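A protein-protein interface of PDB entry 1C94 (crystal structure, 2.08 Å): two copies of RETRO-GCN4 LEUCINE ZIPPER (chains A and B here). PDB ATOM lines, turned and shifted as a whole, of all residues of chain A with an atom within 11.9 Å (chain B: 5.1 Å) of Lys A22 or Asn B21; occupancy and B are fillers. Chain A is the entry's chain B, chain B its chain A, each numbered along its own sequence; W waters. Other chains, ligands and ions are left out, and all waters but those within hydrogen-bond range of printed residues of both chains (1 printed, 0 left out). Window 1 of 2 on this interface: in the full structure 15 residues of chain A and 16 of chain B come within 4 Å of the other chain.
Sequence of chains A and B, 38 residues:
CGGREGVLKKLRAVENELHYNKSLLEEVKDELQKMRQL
The side-chain carboxylate (OE1) of Glu B17 lies close to the side-chain carboxylate (OE2) of Glu A15 (2.5 Å). The side-chain carboxylate (OE1) of Glu A26 is in hydrogen-bond range of the side-chain hydroxyl (OH) of Tyr B20 (2.5 Å).
The side-chain amino group (NZ) of Lys A22 lies within salt-bridge range of the side-chain carboxylate (OE1) of Glu A26.
Leu A18 touches Leu B18 (CD1 to CD1, 3.2 Å). Leu A18 touches Asn B21 (O to OD1, 3.5 Å). Tyr B20 touches Lys A22 (CE2 to NZ, 3.3 Å). CB of Lys A22 touches ND2 of Asn B21, at 3.2 Å. CB of Asn B21 touches CD2 of Leu A25 (3.9 Å). CD2 of Leu B24 touches CB of Leu A25, 3.8 Å away. Leu A25 touches Leu B25. Glu A26 touches Leu B24. CD1 of Leu B24 touches CD of Lys A29 (3.0 Å).
Of the printed residues of chain B, Leu A18 touches Leu B18 (3.2 Å) and Asn B21 (3.5 Å). Lys A22 touches two residues of chain B. Leu A24 touches none of the printed residues of chain B. Of the printed residues of chain B, Leu A25 touches Asn B21 (3.9 Å), Leu B24 (3.8 Å) and Leu B25 (3.5 Å). Printed residues of chain B within 4 Å of Glu A26: Tyr B20 and Leu B24. Glu B17 touches one residue of chain A. Of chain A, only Leu A18 comes within 4 Å of Leu B18. His B19 touches none of the printed residues of chain A. Tyr B20 touches just these residues of chain A: Lys A22 (3.3 Å) and Glu A26 (2.5 Å). Lys B22 touches none of the printed residues of chain A. No residue of chain A comes within 4 Å of Ser B23. Leu B24 touches three residues of chain A. The nearest residue of chain B that does not touch Lys A22 is Leu B24 (4.4 Å). The nearest printed residue of chain B that does not touch Lys A29 is Tyr B20 (6.6 Å).
Printed residues of chain B that touch a printed residue of chain A: Glu B17, Leu B18, Tyr B20, Asn B21, Leu B24 and Leu B25. Hydrophobic or aromatic side chains of chain B that line the printed part of chain A: Leu B18, Tyr B20, Leu B24 and Leu B25.
Leu B18 touches its own counterpart, Leu A18. Leu A25 touches its own counterpart, Leu B25. Glu A26 touches Tyr B20, but with the chains exchanged Tyr A20 does not touch Glu B26 (14.7 Å). Glu A26 touches Leu B24, but with the chains exchanged Leu A24 does not touch Glu B26 (11.8 Å). Of the 11 pairs that touch across the chains among the printed residues, 2 have their exchanged pair printed and touching as well.
Water W1 lies within hydrogen-bond range of the side-chain carboxylate of Glu B17 (2.9 Å) and the side-chain carboxylate of Glu A15 (3.4 Å).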
ATOM      1  N   ALA A  13      19.288 -33.983 -19.601  1.00  0.00           N
ATOM      2  CA  ALA A  13      20.084 -34.151 -20.801  1.00  0.00           C
ATOM      3  C   ALA A  13      19.461 -33.378 -21.916  1.00  0.00           C
ATOM      4  O   ALA A  13      20.091 -32.665 -22.676  1.00  0.00           O
ATOM      5  CB  ALA A  13      20.094 -35.746 -21.156  1.00  0.00           C
ATOM      6  N   VAL A  14      18.152 -33.420 -21.993  1.00  0.00           N
ATOM      7  CA  VAL A  14      17.503 -32.679 -23.072  1.00  0.00           C
ATOM      8  C   VAL A  14      17.727 -31.185 -22.980  1.00  0.00           C
ATOM      9  O   VAL A  14      17.890 -30.455 -23.990  1.00  0.00           O
ATOM     10  CB  VAL A  14      15.963 -32.967 -23.020  1.00  0.00           C
ATOM     11  CG1 VAL A  14      15.164 -31.897 -23.818  1.00  0.00           C
ATOM     12  CG2 VAL A  14      15.711 -34.221 -23.656  1.00  0.00           C
ATOM     13  N   GLU A  15      17.511 -30.659 -21.785  1.00  0.00           N
ATOM     14  CA  GLU A  15      17.724 -29.248 -21.581  1.00  0.00           C
ATOM     15  C   GLU A  15      19.231 -28.888 -21.736  1.00  0.00           C
ATOM     16  O   GLU A  15      19.558 -27.843 -22.358  1.00  0.00           O
ATOM     17  CB  GLU A  15      17.131 -28.841 -20.180  1.00  0.00           C
ATOM     18  CG  GLU A  15      17.216 -27.295 -19.795  1.00  0.00           C
ATOM     19  CD  GLU A  15      18.579 -26.621 -19.698  1.00  0.00           C
ATOM     20  OE1 GLU A  15      19.520 -27.211 -19.138  1.00  0.00           O
ATOM     21  OE2 GLU A  15      18.723 -25.435 -20.178  1.00  0.00           O
ATOM     22  N   ASN A  16      20.179 -29.728 -21.291  1.00  0.00           N
ATOM     23  CA  ASN A  16      21.564 -29.383 -21.593  1.00  0.00           C
ATOM     24  C   ASN A  16      21.826 -29.362 -23.171  1.00  0.00           C
ATOM     25  O   ASN A  16      22.567 -28.486 -23.732  1.00  0.00           O
ATOM     26  CB  ASN A  16      22.546 -30.408 -20.881  1.00  0.00           C
ATOM     27  CG  ASN A  16      22.669 -30.152 -19.350  1.00  0.00           C
ATOM     28  OD1 ASN A  16      22.574 -29.036 -18.900  1.00  0.00           O
ATOM     29  ND2 ASN A  16      22.858 -31.206 -18.559  1.00  0.00           N
ATOM     30  N   GLU A  17      21.315 -30.365 -23.871  1.00  0.00           N
ATOM     31  CA  GLU A  17      21.486 -30.428 -25.328  1.00  0.00           C
ATOM     32  C   GLU A  17      20.851 -29.271 -26.006  1.00  0.00           C
ATOM     33  O   GLU A  17      21.439 -28.726 -26.925  1.00  0.00           O
ATOM     34  CB  GLU A  17      21.039 -31.760 -25.856  1.00  0.00           C
ATOM     35  CG  GLU A  17      21.925 -32.885 -25.357  1.00  0.00           C
ATOM     36  CD  GLU A  17      21.395 -34.241 -25.745  1.00  0.00           C
ATOM     37  OE1 GLU A  17      20.630 -34.364 -26.816  1.00  0.00           O
ATOM     38  OE2 GLU A  17      21.767 -35.200 -25.014  1.00  0.00           O
ATOM     39  N   LEU A  18      19.715 -28.786 -25.508  1.00  0.00           N
ATOM     40  CA  LEU A  18      19.115 -27.586 -26.116  1.00  0.00           C
ATOM     41  C   LEU A  18      20.008 -26.402 -25.864  1.00  0.00           C
ATOM     42  O   LEU A  18      20.127 -25.566 -26.745  1.00  0.00           O
ATOM     43  CB  LEU A  18      17.693 -27.408 -25.429  1.00  0.00           C
ATOM     44  CG  LEU A  18      16.368 -26.797 -25.900  1.00  0.00           C
ATOM     45  CD1 LEU A  18      16.164 -27.019 -27.415  1.00  0.00           C
ATOM     46  CD2 LEU A  18      15.239 -27.443 -24.918  1.00  0.00           C
ATOM     47  N   HIS A  19      20.596 -26.233 -24.621  1.00  0.00           N
ATOM     48  CA  HIS A  19      21.494 -25.062 -24.366  1.00  0.00           C
ATOM     49  C   HIS A  19      22.741 -25.149 -25.290  1.00  0.00           C
ATOM     50  O   HIS A  19      23.303 -24.108 -25.763  1.00  0.00           O
ATOM     51  CB  HIS A  19      21.917 -25.020 -22.891  1.00  0.00           C
ATOM     52  CG  HIS A  19      22.976 -23.995 -22.595  1.00  0.00           C
ATOM     53  ND1 HIS A  19      22.698 -22.689 -22.231  1.00  0.00           N
ATOM     54  CD2 HIS A  19      24.333 -24.042 -22.775  1.00  0.00           C
ATOM     55  CE1 HIS A  19      23.813 -21.973 -22.222  1.00  0.00           C
ATOM     56  NE2 HIS A  19      24.825 -22.762 -22.541  1.00  0.00           N
ATOM     57  N   TYR A  20      23.158 -26.353 -25.616  1.00  0.00           N
ATOM     58  CA  TYR A  20      24.358 -26.462 -26.537  1.00  0.00           C
ATOM     59  C   TYR A  20      23.945 -25.940 -27.932  1.00  0.00           C
ATOM     60  O   TYR A  20      24.719 -25.270 -28.612  1.00  0.00           O
ATOM     61  CB  TYR A  20      24.834 -27.952 -26.614  1.00  0.00           C
ATOM     62  CG  TYR A  20      25.951 -28.171 -27.607  1.00  0.00           C
ATOM     63  CD1 TYR A  20      27.306 -28.075 -27.249  1.00  0.00           C
ATOM     64  CD2 TYR A  20      25.676 -28.369 -28.953  1.00  0.00           C
ATOM     65  CE1 TYR A  20      28.361 -28.149 -28.257  1.00  0.00           C
ATOM     66  CE2 TYR A  20      26.731 -28.462 -29.932  1.00  0.00           C
ATOM     67  CZ  TYR A  20      28.044 -28.338 -29.580  1.00  0.00           C
ATOM     68  OH  TYR A  20      29.049 -28.379 -30.601  1.00  0.00           O
ATOM     69  N   ASN A  21      22.778 -26.315 -28.395  1.00  0.00           N
ATOM     70  CA  ASN A  21      22.292 -25.822 -29.762  1.00  0.00           C
ATOM     71  C   ASN A  21      22.095 -24.376 -29.637  1.00  0.00           C
ATOM     72  O   ASN A  21      22.328 -23.599 -30.557  1.00  0.00           O
ATOM     73  CB  ASN A  21      20.914 -26.504 -30.112  1.00  0.00           C
ATOM     74  CG  ASN A  21      21.060 -27.909 -30.569  1.00  0.00           C
ATOM     75  OD1 ASN A  21      20.060 -28.633 -30.871  1.00  0.00           O
ATOM     76  ND2 ASN A  21      22.262 -28.326 -30.657  1.00  0.00           N
ATOM     77  N   LYS A  22      21.607 -23.899 -28.503  1.00  0.00           N
ATOM     78  CA  LYS A  22      21.526 -22.422 -28.351  1.00  0.00           C
ATOM     79  C   LYS A  22      22.833 -21.621 -28.497  1.00  0.00           C
ATOM     80  O   LYS A  22      22.902 -20.535 -29.132  1.00  0.00           O
ATOM     81  CB  LYS A  22      20.740 -22.053 -27.024  1.00  0.00           C
ATOM     82  CG  LYS A  22      20.869 -20.497 -26.580  1.00  0.00           C
ATOM     83  CD  LYS A  22      20.306 -20.164 -25.241  1.00  0.00           C
ATOM     84  CE  LYS A  22      20.962 -19.025 -24.618  1.00  0.00           C
ATOM     85  NZ  LYS A  22      21.263 -17.971 -25.627  1.00  0.00           N
ATOM     86  N   SER A  23      23.936 -22.077 -27.901  1.00  0.00           N
ATOM     87  CA  SER A  23      25.254 -21.378 -28.001  1.00  0.00           C
ATOM     88  C   SER A  23      25.741 -21.509 -29.461  1.00  0.00           C
ATOM     89  O   SER A  23      26.399 -20.616 -29.980  1.00  0.00           O
ATOM     90  CB  SER A  23      26.323 -22.043 -27.123  1.00  0.00           C
ATOM     91  OG  SER A  23      25.714 -22.263 -25.833  1.00  0.00           O
ATOM     92  N   LEU A  24      25.461 -22.643 -30.086  1.00  0.00           N
ATOM     93  CA  LEU A  24      25.893 -22.740 -31.482  1.00  0.00           C
ATOM     94  C   LEU A  24      25.138 -21.788 -32.410  1.00  0.00           C
ATOM     95  O   LEU A  24      25.702 -21.115 -33.312  1.00  0.00           O
ATOM     96  CB  LEU A  24      25.720 -24.119 -31.894  1.00  0.00           C
ATOM     97  CG  LEU A  24      26.370 -24.657 -33.115  1.00  0.00           C
ATOM     98  CD1 LEU A  24      27.880 -24.196 -33.118  1.00  0.00           C
ATOM     99  CD2 LEU A  24      26.131 -26.245 -33.024  1.00  0.00           C
ATOM    100  N   LEU A  25      23.828 -21.713 -32.193  1.00  0.00           N
ATOM    101  CA  LEU A  25      22.954 -20.812 -32.983  1.00  0.00           C
ATOM    102  C   LEU A  25      23.409 -19.428 -32.761  1.00  0.00           C
ATOM    103  O   LEU A  25      23.337 -18.649 -33.681  1.00  0.00           O
ATOM    104  CB  LEU A  25      21.523 -20.976 -32.473  1.00  0.00           C
ATOM    105  CG  LEU A  25      20.249 -20.908 -33.303  1.00  0.00           C
ATOM    106  CD1 LEU A  25      20.355 -21.143 -34.890  1.00  0.00           C
ATOM    107  CD2 LEU A  25      19.475 -22.016 -32.616  1.00  0.00           C
ATOM    108  N   GLU A  26      23.764 -19.019 -31.522  1.00  0.00           N
ATOM    109  CA  GLU A  26      24.270 -17.646 -31.307  1.00  0.00           C
ATOM    110  C   GLU A  26      25.627 -17.437 -32.057  1.00  0.00           C
ATOM    111  O   GLU A  26      25.949 -16.349 -32.533  1.00  0.00           O
ATOM    112  CB  GLU A  26      24.562 -17.342 -29.820  1.00  0.00           C
ATOM    113  CG  GLU A  26      23.459 -17.447 -28.831  1.00  0.00           C
ATOM    114  CD  GLU A  26      22.559 -16.278 -28.688  1.00  0.00           C
ATOM    115  OE1 GLU A  26      21.778 -16.259 -27.713  1.00  0.00           O
ATOM    116  OE2 GLU A  26      22.597 -15.369 -29.479  1.00  0.00           O
ATOM    117  N   GLU A  27      26.424 -18.488 -32.087  1.00  0.00           N
ATOM    118  CA  GLU A  27      27.688 -18.467 -32.805  1.00  0.00           C
ATOM    119  C   GLU A  27      27.390 -18.292 -34.315  1.00  0.00           C
ATOM    120  O   GLU A  27      28.069 -17.443 -35.016  1.00  0.00           O
ATOM    121  CB  GLU A  27      28.494 -19.747 -32.572  1.00  0.00           C
ATOM    122  CG  GLU A  27      29.603 -19.986 -33.684  1.00  0.00           C
ATOM    123  CD  GLU A  27      30.584 -21.207 -33.450  1.00  0.00           C
ATOM    124  OE1 GLU A  27      30.164 -22.283 -32.953  1.00  0.00           O
ATOM    125  OE2 GLU A  27      31.790 -21.100 -33.803  1.00  0.00           O
ATOM    126  N   VAL A  28      26.383 -18.983 -34.832  1.00  0.00           N
ATOM    127  CA  VAL A  28      25.997 -18.790 -36.270  1.00  0.00           C
ATOM    128  C   VAL A  28      25.543 -17.386 -36.455  1.00  0.00           C
ATOM    129  O   VAL A  28      25.922 -16.680 -37.359  1.00  0.00           O
ATOM    130  CB  VAL A  28      24.790 -19.722 -36.648  1.00  0.00           C
ATOM    131  CG1 VAL A  28      24.159 -19.247 -38.083  1.00  0.00           C
ATOM    132  CG2 VAL A  28      25.281 -21.067 -36.799  1.00  0.00           C
ATOM    133  N   LYS A  29      24.597 -16.944 -35.661  1.00  0.00           N
ATOM    134  CA  LYS A  29      24.166 -15.571 -35.774  1.00  0.00           C
ATOM    135  C   LYS A  29      25.322 -14.544 -35.699  1.00  0.00           C
ATOM    136  O   LYS A  29      25.331 -13.556 -36.454  1.00  0.00           O
ATOM    137  CB  LYS A  29      23.259 -15.244 -34.625  1.00  0.00           C
ATOM    138  CG  LYS A  29      22.256 -14.098 -34.916  1.00  0.00           C
ATOM    139  CD  LYS A  29      21.544 -13.812 -33.648  1.00  0.00           C
ATOM    140  CE  LYS A  29      22.432 -13.089 -32.748  1.00  0.00           C
ATOM    141  NZ  LYS A  29      22.646 -11.904 -33.556  1.00  0.00           N
ATOM    142  N   ASP A  30      26.230 -14.704 -34.728  1.00  0.00           N
ATOM    143  CA  ASP A  30      27.338 -13.730 -34.584  1.00  0.00           C
ATOM    144  C   ASP A  30      28.163 -13.808 -35.860  1.00  0.00           C
ATOM    145  O   ASP A  30      28.644 -12.822 -36.327  1.00  0.00           O
ATOM    146  CB  ASP A  30      28.360 -14.013 -33.417  1.00  0.00           C
ATOM    147  CG  ASP A  30      27.734 -14.070 -32.004  1.00  0.00           C
ATOM    148  OD1 ASP A  30      26.648 -13.476 -31.785  1.00  0.00           O
ATOM    149  OD2 ASP A  30      28.378 -14.719 -31.114  1.00  0.00           O
ATOM    150  N   GLU A  31      28.378 -15.005 -36.384  1.00  0.00           N
ATOM    151  CA  GLU A  31      29.187 -15.098 -37.573  1.00  0.00           C
ATOM    152  C   GLU A  31      28.524 -14.522 -38.725  1.00  0.00           C
ATOM    153  O   GLU A  31      29.175 -14.024 -39.633  1.00  0.00           O
ATOM    154  CB  GLU A  31      29.598 -16.522 -37.857  1.00  0.00           C
ATOM    155  CG  GLU A  31      30.733 -16.919 -36.873  1.00  0.00           C
ATOM    156  CD  GLU A  31      31.004 -18.386 -36.879  1.00  0.00           C
ATOM    157  OE1 GLU A  31      31.665 -18.849 -35.889  1.00  0.00           O
ATOM    158  OE2 GLU A  31      30.543 -19.048 -37.883  1.00  0.00           O
ATOM    159  N   LEU A  32      27.210 -14.542 -38.731  1.00  0.00           N
ATOM    160  CA  LEU A  32      26.528 -13.921 -39.874  1.00  0.00           C
ATOM    161  C   LEU A  32      26.556 -12.415 -39.793  1.00  0.00           C
ATOM    162  O   LEU A  32      26.710 -11.694 -40.794  1.00  0.00           O
ATOM    163  CB  LEU A  32      25.059 -14.290 -39.877  1.00  0.00           C
ATOM    164  CG  LEU A  32      24.665 -15.538 -40.584  1.00  0.00           C
ATOM    165  CD1 LEU A  32      23.133 -15.517 -40.443  1.00  0.00           C
ATOM    166  CD2 LEU A  32      25.064 -15.530 -42.099  1.00  0.00           C
ATOM    167  N   GLU B  17      12.995 -22.540 -23.694  1.00  0.00           N
ATOM    168  CA  GLU B  17      14.308 -22.557 -24.321  1.00  0.00           C
ATOM    169  C   GLU B  17      14.216 -22.877 -25.755  1.00  0.00           C
ATOM    170  O   GLU B  17      14.871 -22.187 -26.606  1.00  0.00           O
ATOM    171  CB  GLU B  17      15.208 -23.493 -23.536  1.00  0.00           C
ATOM    172  CG  GLU B  17      15.455 -22.890 -22.133  1.00  0.00           C
ATOM    173  CD  GLU B  17      16.379 -23.728 -21.287  1.00  0.00           C
ATOM    174  OE1 GLU B  17      17.210 -24.571 -21.951  1.00  0.00           O
ATOM    175  OE2 GLU B  17      16.267 -23.533 -19.995  1.00  0.00           O
ATOM    176  N   LEU B  18      13.302 -23.788 -26.125  1.00  0.00           N
ATOM    177  CA  LEU B  18      13.095 -24.102 -27.580  1.00  0.00           C
ATOM    178  C   LEU B  18      12.503 -22.933 -28.302  1.00  0.00           C
ATOM    179  O   LEU B  18      12.865 -22.621 -29.482  1.00  0.00           O
ATOM    180  CB  LEU B  18      12.104 -25.289 -27.619  1.00  0.00           C
ATOM    181  CG  LEU B  18      11.987 -26.488 -28.602  1.00  0.00           C
ATOM    182  CD1 LEU B  18      13.402 -26.895 -29.113  1.00  0.00           C
ATOM    183  CD2 LEU B  18      11.147 -27.684 -27.843  1.00  0.00           C
ATOM    184  N   HIS B  19      11.525 -22.191 -27.671  1.00  0.00           N
ATOM    185  CA  HIS B  19      10.994 -21.029 -28.352  1.00  0.00           C
ATOM    186  C   HIS B  19      12.102 -19.924 -28.519  1.00  0.00           C
ATOM    187  O   HIS B  19      12.218 -19.208 -29.576  1.00  0.00           O
ATOM    188  CB  HIS B  19       9.768 -20.471 -27.604  1.00  0.00           C
ATOM    189  CG  HIS B  19       9.310 -19.118 -28.116  1.00  0.00           C
ATOM    190  ND1 HIS B  19       8.337 -18.979 -29.092  1.00  0.00           N
ATOM    191  CD2 HIS B  19       9.782 -17.872 -27.888  1.00  0.00           C
ATOM    192  CE1 HIS B  19       8.233 -17.712 -29.470  1.00  0.00           C
ATOM    193  NE2 HIS B  19       9.102 -17.007 -28.763  1.00  0.00           N
ATOM    194  N   TYR B  20      13.019 -19.858 -27.577  1.00  0.00           N
ATOM    195  CA  TYR B  20      14.140 -18.851 -27.757  1.00  0.00           C
ATOM    196  C   TYR B  20      15.000 -19.261 -29.035  1.00  0.00           C
ATOM    197  O   TYR B  20      15.461 -18.433 -29.872  1.00  0.00           O
ATOM    198  CB  TYR B  20      15.002 -18.833 -26.461  1.00  0.00           C
ATOM    199  CG  TYR B  20      16.209 -17.910 -26.539  1.00  0.00           C
ATOM    200  CD1 TYR B  20      16.164 -16.563 -26.158  1.00  0.00           C
ATOM    201  CD2 TYR B  20      17.379 -18.357 -27.152  1.00  0.00           C
ATOM    202  CE1 TYR B  20      17.278 -15.685 -26.416  1.00  0.00           C
ATOM    203  CE2 TYR B  20      18.476 -17.465 -27.374  1.00  0.00           C
ATOM    204  CZ  TYR B  20      18.410 -16.156 -27.020  1.00  0.00           C
ATOM    205  OH  TYR B  20      19.527 -15.340 -27.308  1.00  0.00           O
ATOM    206  N   ASN B  21      15.227 -20.518 -29.217  1.00  0.00           N
ATOM    207  CA  ASN B  21      16.098 -20.969 -30.341  1.00  0.00           C
ATOM    208  C   ASN B  21      15.305 -20.775 -31.569  1.00  0.00           C
ATOM    209  O   ASN B  21      15.810 -20.434 -32.670  1.00  0.00           O
ATOM    210  CB  ASN B  21      16.423 -22.509 -30.206  1.00  0.00           C
ATOM    211  CG  ASN B  21      17.463 -22.826 -29.164  1.00  0.00           C
ATOM    212  OD1 ASN B  21      17.786 -24.018 -28.892  1.00  0.00           O
ATOM    213  ND2 ASN B  21      17.977 -21.814 -28.546  1.00  0.00           N
ATOM    214  N   LYS B  22      14.002 -21.010 -31.467  1.00  0.00           N
ATOM    215  CA  LYS B  22      13.164 -20.713 -32.630  1.00  0.00           C
ATOM    216  C   LYS B  22      13.262 -19.278 -33.122  1.00  0.00           C
ATOM    217  O   LYS B  22      13.324 -19.043 -34.349  1.00  0.00           O
ATOM    218  CB  LYS B  22      11.641 -21.110 -32.356  1.00  0.00           C
ATOM    219  CG  LYS B  22      10.577 -20.495 -33.470  1.00  0.00           C
ATOM    220  CD  LYS B  22       9.114 -20.852 -33.191  1.00  0.00           C
ATOM    221  CE  LYS B  22       8.185 -19.792 -33.619  1.00  0.00           C
ATOM    222  NZ  LYS B  22       8.591 -19.331 -34.973  1.00  0.00           N
ATOM    223  N   SER B  23      13.176 -18.261 -32.237  1.00  0.00           N
ATOM    224  CA  SER B  23      13.230 -16.818 -32.677  1.00  0.00           C
ATOM    225  C   SER B  23      14.686 -16.602 -33.192  1.00  0.00           C
ATOM    226  O   SER B  23      14.997 -15.835 -34.164  1.00  0.00           O
ATOM    227  CB  SER B  23      13.035 -15.828 -31.473  1.00  0.00           C
ATOM    228  OG  SER B  23      11.928 -16.260 -30.631  1.00  0.00           O
ATOM    229  N   LEU B  24      15.670 -17.163 -32.531  1.00  0.00           N
ATOM    230  CA  LEU B  24      16.976 -16.864 -33.122  1.00  0.00           C
ATOM    231  C   LEU B  24      17.194 -17.436 -34.521  1.00  0.00           C
ATOM    232  O   LEU B  24      17.964 -16.891 -35.439  1.00  0.00           O
ATOM    233  CB  LEU B  24      17.945 -17.399 -32.152  1.00  0.00           C
ATOM    234  CG  LEU B  24      19.382 -17.110 -32.238  1.00  0.00           C
ATOM    235  CD1 LEU B  24      19.559 -15.576 -32.321  1.00  0.00           C
ATOM    236  CD2 LEU B  24      19.988 -17.796 -30.980  1.00  0.00           C
ATOM    237  N   LEU B  25      16.610 -18.601 -34.730  1.00  0.00           N
ATOM    238  CA  LEU B  25      16.723 -19.325 -36.038  1.00  0.00           C
ATOM    239  C   LEU B  25      15.990 -18.503 -37.021  1.00  0.00           C
ATOM    240  O   LEU B  25      16.440 -18.382 -38.153  1.00  0.00           O
ATOM    241  CB  LEU B  25      16.059 -20.706 -35.877  1.00  0.00           C
ATOM    242  CG  LEU B  25      16.446 -21.951 -36.607  1.00  0.00           C
ATOM    243  CD1 LEU B  25      17.911 -21.994 -37.197  1.00  0.00           C
ATOM    244  CD2 LEU B  25      16.233 -22.940 -35.480  1.00  0.00           C
ATOM    245  N   GLU B  26      14.837 -17.901 -36.670  1.00  0.00           N
ATOM    246  CA  GLU B  26      14.147 -17.027 -37.647  1.00  0.00           C
ATOM    247  C   GLU B  26      14.960 -15.776 -37.923  1.00  0.00           C
ATOM    248  O   GLU B  26      14.912 -15.175 -39.018  1.00  0.00           O
ATOM    249  CB  GLU B  26      12.836 -16.531 -37.080  1.00  0.00           C
ATOM    250  CG  GLU B  26      11.746 -17.545 -36.674  1.00  0.00           C
ATOM    251  CD  GLU B  26      10.854 -18.021 -37.796  1.00  0.00           C
ATOM    252  OE1 GLU B  26       9.831 -18.719 -37.490  1.00  0.00           O
ATOM    253  OE2 GLU B  26      11.132 -17.734 -38.972  1.00  0.00           O
HETATM  254  O   HOH W   1      16.942 -24.630 -17.373  1.00  0.00           O
